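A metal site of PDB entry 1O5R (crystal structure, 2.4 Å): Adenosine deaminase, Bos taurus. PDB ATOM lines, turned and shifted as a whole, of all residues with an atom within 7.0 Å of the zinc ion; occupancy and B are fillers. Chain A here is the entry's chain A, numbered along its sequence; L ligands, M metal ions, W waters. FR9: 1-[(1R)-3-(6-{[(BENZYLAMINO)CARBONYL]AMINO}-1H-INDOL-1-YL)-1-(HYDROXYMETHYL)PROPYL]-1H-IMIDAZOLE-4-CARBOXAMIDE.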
ATOM      1  N   HIS A  14      -8.875  -0.315  -5.157  1.00  0.00           N
ATOM      2  CA  HIS A  14     -10.060  -0.231  -4.318  1.00  0.00           C
ATOM      3  C   HIS A  14     -10.424   1.249  -3.815  1.00  0.00           C
ATOM      4  O   HIS A  14      -9.896   1.697  -2.776  1.00  0.00           O
ATOM      5  CB  HIS A  14     -10.199  -1.037  -3.014  1.00  0.00           C
ATOM      6  CG  HIS A  14     -11.461  -1.268  -2.226  1.00  0.00           C
ATOM      7  ND1 HIS A  14     -11.699  -2.546  -1.837  1.00  0.00           N
ATOM      8  CD2 HIS A  14     -12.598  -0.497  -1.932  1.00  0.00           C
ATOM      9  CE1 HIS A  14     -12.936  -2.543  -1.316  1.00  0.00           C
ATOM     10  NE2 HIS A  14     -13.499  -1.334  -1.359  1.00  0.00           N
ATOM     11  N   VAL A  15     -11.159   1.968  -4.573  1.00  0.00           N
ATOM     12  CA  VAL A  15     -11.459   3.342  -4.234  1.00  0.00           C
ATOM     13  C   VAL A  15     -12.846   3.615  -4.816  1.00  0.00           C
ATOM     14  O   VAL A  15     -13.128   3.285  -5.929  1.00  0.00           O
ATOM     15  CB  VAL A  15     -10.384   4.405  -4.723  1.00  0.00           C
ATOM     16  CG1 VAL A  15     -10.075   4.235  -6.211  1.00  0.00           C
ATOM     17  CG2 VAL A  15     -10.943   5.806  -4.361  1.00  0.00           C
ATOM     18  N   HIS A  16     -13.690   4.195  -3.987  1.00  0.00           N
ATOM     19  CA  HIS A  16     -15.031   4.414  -4.515  1.00  0.00           C
ATOM     20  C   HIS A  16     -15.347   5.801  -5.121  1.00  0.00           C
ATOM     21  O   HIS A  16     -15.228   6.756  -4.394  1.00  0.00           O
ATOM     22  CB  HIS A  16     -16.018   4.221  -3.319  1.00  0.00           C
ATOM     23  CG  HIS A  16     -16.160   2.825  -2.766  1.00  0.00           C
ATOM     24  ND1 HIS A  16     -17.197   2.042  -3.098  1.00  0.00           N
ATOM     25  CD2 HIS A  16     -15.380   2.178  -1.884  1.00  0.00           C
ATOM     26  CE1 HIS A  16     -17.034   0.880  -2.362  1.00  0.00           C
ATOM     27  NE2 HIS A  16     -15.919   0.954  -1.647  1.00  0.00           N
ATOM     28  N   ARG A 100     -14.356   2.339  -8.320  1.00  0.00           N
ATOM     29  CA  ARG A 100     -15.633   1.644  -8.279  1.00  0.00           C
ATOM     30  C   ARG A 100     -16.789   2.510  -7.783  1.00  0.00           C
ATOM     31  O   ARG A 100     -16.624   3.458  -7.033  1.00  0.00           O
ATOM     32  CB  ARG A 100     -15.476   0.398  -7.406  1.00  0.00           C
ATOM     33  CG  ARG A 100     -15.860   0.625  -5.940  1.00  0.00           C
ATOM     34  CD  ARG A 100     -15.504  -0.618  -5.137  1.00  0.00           C
ATOM     35  NE  ARG A 100     -14.929  -1.611  -6.059  1.00  0.00           N
ATOM     36  CZ  ARG A 100     -13.899  -2.350  -5.624  1.00  0.00           C
ATOM     37  NH1 ARG A 100     -13.558  -2.328  -4.345  1.00  0.00           N
ATOM     38  NH2 ARG A 100     -13.083  -2.901  -6.521  1.00  0.00           N
ATOM     39  N   ASP A 180     -18.678  -5.682  -8.894  1.00  0.00           N
ATOM     40  CA  ASP A 180     -18.348  -5.693  -7.473  1.00  0.00           C
ATOM     41  C   ASP A 180     -19.595  -5.831  -6.583  1.00  0.00           C
ATOM     42  O   ASP A 180     -20.732  -5.778  -7.035  1.00  0.00           O
ATOM     43  CB  ASP A 180     -17.607  -4.401  -7.135  1.00  0.00           C
ATOM     44  CG  ASP A 180     -17.239  -4.392  -5.659  1.00  0.00           C
ATOM     45  OD1 ASP A 180     -17.407  -3.351  -5.028  1.00  0.00           O
ATOM     46  OD2 ASP A 180     -16.780  -5.418  -5.155  1.00  0.00           O
ATOM     47  N   ALA A 182     -21.261  -4.604  -2.781  1.00  0.00           N
ATOM     48  CA  ALA A 182     -21.251  -3.854  -1.530  1.00  0.00           C
ATOM     49  C   ALA A 182     -22.377  -2.814  -1.523  1.00  0.00           C
ATOM     50  O   ALA A 182     -22.899  -2.406  -2.550  1.00  0.00           O
ATOM     51  CB  ALA A 182     -19.899  -3.172  -1.367  1.00  0.00           C
ATOM     52  N   HIS A 213     -16.762  -7.291  -1.851  1.00  0.00           N
ATOM     53  CA  HIS A 213     -16.582  -6.786  -0.495  1.00  0.00           C
ATOM     54  C   HIS A 213     -16.934  -7.871   0.524  1.00  0.00           C
ATOM     55  O   HIS A 213     -18.095  -8.218   0.719  1.00  0.00           O
ATOM     56  CB  HIS A 213     -17.511  -5.592  -0.297  1.00  0.00           C
ATOM     57  CG  HIS A 213     -16.813  -4.325  -0.732  1.00  0.00           C
ATOM     58  ND1 HIS A 213     -16.884  -3.837  -1.983  1.00  0.00           N
ATOM     59  CD2 HIS A 213     -16.115  -3.408   0.068  1.00  0.00           C
ATOM     60  CE1 HIS A 213     -16.254  -2.648  -1.949  1.00  0.00           C
ATOM     61  NE2 HIS A 213     -15.780  -2.363  -0.727  1.00  0.00           N
ATOM     62  N   GLU A 216     -14.810  -7.514   5.692  1.00  0.00           N
ATOM     63  CA  GLU A 216     -14.496  -6.219   6.298  1.00  0.00           C
ATOM     64  C   GLU A 216     -15.125  -6.097   7.689  1.00  0.00           C
ATOM     65  O   GLU A 216     -14.469  -5.824   8.686  1.00  0.00           O
ATOM     66  CB  GLU A 216     -15.013  -5.114   5.376  1.00  0.00           C
ATOM     67  CG  GLU A 216     -15.018  -3.746   6.057  1.00  0.00           C
ATOM     68  CD  GLU A 216     -15.630  -2.724   5.124  1.00  0.00           C
ATOM     69  OE1 GLU A 216     -16.230  -3.117   4.136  1.00  0.00           O
ATOM     70  OE2 GLU A 216     -15.493  -1.532   5.393  1.00  0.00           O
ATOM     71  N   GLY A 236     -12.389  -7.876  -1.274  1.00  0.00           N
ATOM     72  CA  GLY A 236     -12.378  -6.525  -0.739  1.00  0.00           C
ATOM     73  C   GLY A 236     -12.194  -6.547   0.781  1.00  0.00           C
ATOM     74  O   GLY A 236     -13.078  -6.925   1.545  1.00  0.00           O
ATOM     75  N   HIS A 237     -10.988  -6.146   1.226  1.00  0.00           N
ATOM     76  CA  HIS A 237     -10.678  -6.253   2.642  1.00  0.00           C
ATOM     77  C   HIS A 237     -10.267  -7.682   3.006  1.00  0.00           C
ATOM     78  O   HIS A 237      -9.101  -8.008   3.146  1.00  0.00           O
ATOM     79  CB  HIS A 237     -11.941  -5.863   3.428  1.00  0.00           C
ATOM     80  CG  HIS A 237     -12.265  -4.420   3.185  1.00  0.00           C
ATOM     81  ND1 HIS A 237     -11.593  -3.396   3.753  1.00  0.00           N
ATOM     82  CD2 HIS A 237     -13.327  -3.889   2.434  1.00  0.00           C
ATOM     83  CE1 HIS A 237     -12.229  -2.276   3.368  1.00  0.00           C
ATOM     84  NE2 HIS A 237     -13.272  -2.539   2.580  1.00  0.00           N
ATOM     85  N   GLU A 259      -7.552  -6.741  -1.241  1.00  0.00           N
ATOM     86  CA  GLU A 259      -7.544  -5.240  -1.259  1.00  0.00           C
ATOM     87  C   GLU A 259      -7.782  -4.605   0.146  1.00  0.00           C
ATOM     88  O   GLU A 259      -8.866  -4.315   0.609  1.00  0.00           O
ATOM     89  CB  GLU A 259      -8.624  -4.668  -2.177  1.00  0.00           C
ATOM     90  CG  GLU A 259      -8.735  -5.386  -3.536  1.00  0.00           C
ATOM     91  CD  GLU A 259     -10.136  -5.225  -4.165  1.00  0.00           C
ATOM     92  OE1 GLU A 259     -10.330  -5.752  -5.235  1.00  0.00           O
ATOM     93  OE2 GLU A 259     -11.053  -4.621  -3.615  1.00  0.00           O
ATOM     94  N   CYS A 261      -7.693  -1.942   3.170  1.00  0.00           N
ATOM     95  CA  CYS A 261      -7.751  -0.515   3.296  1.00  0.00           C
ATOM     96  C   CYS A 261      -7.474  -0.065   4.758  1.00  0.00           C
ATOM     97  O   CYS A 261      -8.396  -0.012   5.567  1.00  0.00           O
ATOM     98  CB  CYS A 261      -9.172  -0.119   2.942  1.00  0.00           C
ATOM     99  SG  CYS A 261      -9.600  -0.603   1.227  1.00  0.00           S
ATOM    100  N   SER A 264      -9.322   3.188   6.130  1.00  0.00           N
ATOM    101  CA  SER A 264     -10.639   2.765   6.265  1.00  0.00           C
ATOM    102  C   SER A 264     -10.943   1.849   7.386  1.00  0.00           C
ATOM    103  O   SER A 264     -11.835   2.172   8.132  1.00  0.00           O
ATOM    104  CB  SER A 264     -11.155   2.152   5.010  1.00  0.00           C
ATOM    105  OG  SER A 264     -12.574   1.890   5.076  1.00  0.00           O
ATOM    106  N   ASP A 294     -10.231   3.613  -0.290  1.00  0.00           N
ATOM    107  CA  ASP A 294     -11.621   3.349  -0.103  1.00  0.00           C
ATOM    108  C   ASP A 294     -12.417   4.564  -0.373  1.00  0.00           C
ATOM    109  O   ASP A 294     -13.096   4.724  -1.371  1.00  0.00           O
ATOM    110  CB  ASP A 294     -11.883   2.626   1.225  1.00  0.00           C
ATOM    111  CG  ASP A 294     -13.023   1.604   1.431  1.00  0.00           C
ATOM    112  OD1 ASP A 294     -13.369   1.232   2.573  1.00  0.00           O
ATOM    113  OD2 ASP A 294     -13.466   1.165   0.375  1.00  0.00           O
ATOM    114  N   ASP A 295     -12.294   5.476   0.568  1.00  0.00           N
ATOM    115  CA  ASP A 295     -13.090   6.689   0.483  1.00  0.00           C
ATOM    116  C   ASP A 295     -12.298   7.882   0.965  1.00  0.00           C
ATOM    117  O   ASP A 295     -12.444   8.295   2.110  1.00  0.00           O
ATOM    118  CB  ASP A 295     -14.383   6.751   1.330  1.00  0.00           C
ATOM    119  CG  ASP A 295     -15.384   5.638   0.939  1.00  0.00           C
ATOM    120  OD1 ASP A 295     -16.403   5.832   0.194  1.00  0.00           O
ATOM    121  OD2 ASP A 295     -15.191   4.527   1.395  1.00  0.00           O
HETATM  122  C1  FR9 L   1     -19.530   1.998   0.027  1.00  0.00           C
HETATM  123  N2  FR9 L   1     -19.821   3.038  -0.985  1.00  0.00           N
HETATM  124  C3  FR9 L   1     -18.961   3.985  -0.651  1.00  0.00           C
HETATM  125  N4  FR9 L   1     -18.143   3.711   0.327  1.00  0.00           N
HETATM  126  C5  FR9 L   1     -18.489   2.376   0.805  1.00  0.00           C
HETATM  127  C8  FR9 L   1     -17.755   1.673   1.846  1.00  0.00           C
HETATM  128  O9  FR9 L   1     -18.135   0.644   2.036  1.00  0.00           O
HETATM  129  N10 FR9 L   1     -16.895   2.263   2.506  1.00  0.00           N
HETATM  130  C13 FR9 L   1     -20.943   3.161  -1.909  1.00  0.00           C
HETATM  131  C14 FR9 L   1     -20.679   2.607  -3.351  1.00  0.00           C
HETATM  132  O15 FR9 L   1     -19.498   2.977  -4.207  1.00  0.00           O
HETATM  133  C18 FR9 L   1     -22.179   2.495  -1.354  1.00  0.00           C
HETATM  134  C19 FR9 L   1     -22.933   3.407  -0.392  1.00  0.00           C
HETATM  135  N22 FR9 L   1     -23.904   2.632   0.341  1.00  0.00           N
HETATM  136  C27 FR9 L   1     -25.256   2.630   0.069  1.00  0.00           C
HETATM  137  C28 FR9 L   1     -25.885   1.735   0.887  1.00  0.00           C
HETATM  138  C29 FR9 L   1     -24.852   1.191   1.697  1.00  0.00           C
HETATM  139  C30 FR9 L   1     -23.636   1.791   1.314  1.00  0.00           C
HETATM  140  C31 FR9 L   1     -24.866   0.312   2.747  1.00  0.00           C
HETATM  141  C32 FR9 L   1     -23.670  -0.006   3.393  1.00  0.00           C
HETATM  142  C33 FR9 L   1     -22.480   0.581   2.958  1.00  0.00           C
HETATM  143  C34 FR9 L   1     -22.500   1.483   1.924  1.00  0.00           C
HETATM  144  N1  FR9 L   1     -21.316   0.461   3.545  1.00  0.00           N
HETATM  145  C2  FR9 L   1     -20.969  -0.455   4.484  1.00  0.00           C
HETATM  146  O1  FR9 L   1     -21.809  -1.106   5.043  1.00  0.00           O
HETATM  147  N3  FR9 L   1     -19.748  -0.289   4.874  1.00  0.00           N
HETATM  148  C6  FR9 L   1     -19.231  -0.985   6.023  1.00  0.00           C
HETATM  149  C7  FR9 L   1     -18.817   1.327   6.950  1.00  0.00           C
HETATM  150  C11 FR9 L   1     -19.173   0.012   7.169  1.00  0.00           C
HETATM  151  C9  FR9 L   1     -19.457  -0.407   8.458  1.00  0.00           C
HETATM  152  C12 FR9 L   1     -19.439   0.510   9.503  1.00  0.00           C
HETATM  153  C10 FR9 L   1     -19.104   1.860   9.287  1.00  0.00           C
HETATM  154  C15 FR9 L   1     -18.754   2.205   8.025  1.00  0.00           C
HETATM  155 ZN    ZN M   1     -15.073  -0.298  -0.448  1.00  0.00          ZN
HETATM  156  O   HOH W   1     -15.259  -0.240   1.345  1.00  0.00           O
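Of the 15 residues printed, 4 come within 4 Å of the zinc ion. Along chain A the residues within 4 Å of the zinc ion span positions 14 to 294.
Water W1 lies within hydrogen-bond range of the side-chain carboxylate of Asp 294, an oxygen (O9) of the ligand and a ring nitrogen (NE2) of His 237.
The zinc ion is bound by water W1, at 1.8 Å. The zinc ion is bound by NE2 of His 16. The zinc ion is bound by a ring nitrogen (NE2) of His 14, 2.1 Å away. The zinc ion is bound by NE2 of His 213, at 2.2 Å. OD2 of Asp 294 is bound to the zinc ion, at 2.3 Å. The zinc ion has five donor atoms within binding distance.
A ring nitrogen (ND1) of His 14 lies close to the guanidinium group (NH1) of Arg 100, at 3.1 Å. OE2 of Glu 259 sits at hydrogen-bond distance from ND1 of His 14 (2.8 Å). OD1 of Asp 180 sits at hydrogen-bond distance from ND1 of His 213 (3.1 Å). OD1 of Asp 294 lies within hydrogen-bond range of OG of Ser 264 (2.7 Å).
An oxygen (O15) of the ligand lies within hydrogen-bond range of a ring nitrogen (ND1) of His 16 (2.7 Å). The side-chain carboxylate (OD1) of Asp 295 is in hydrogen-bond range of a nitrogen (N4) of the ligand (2.7 Å).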
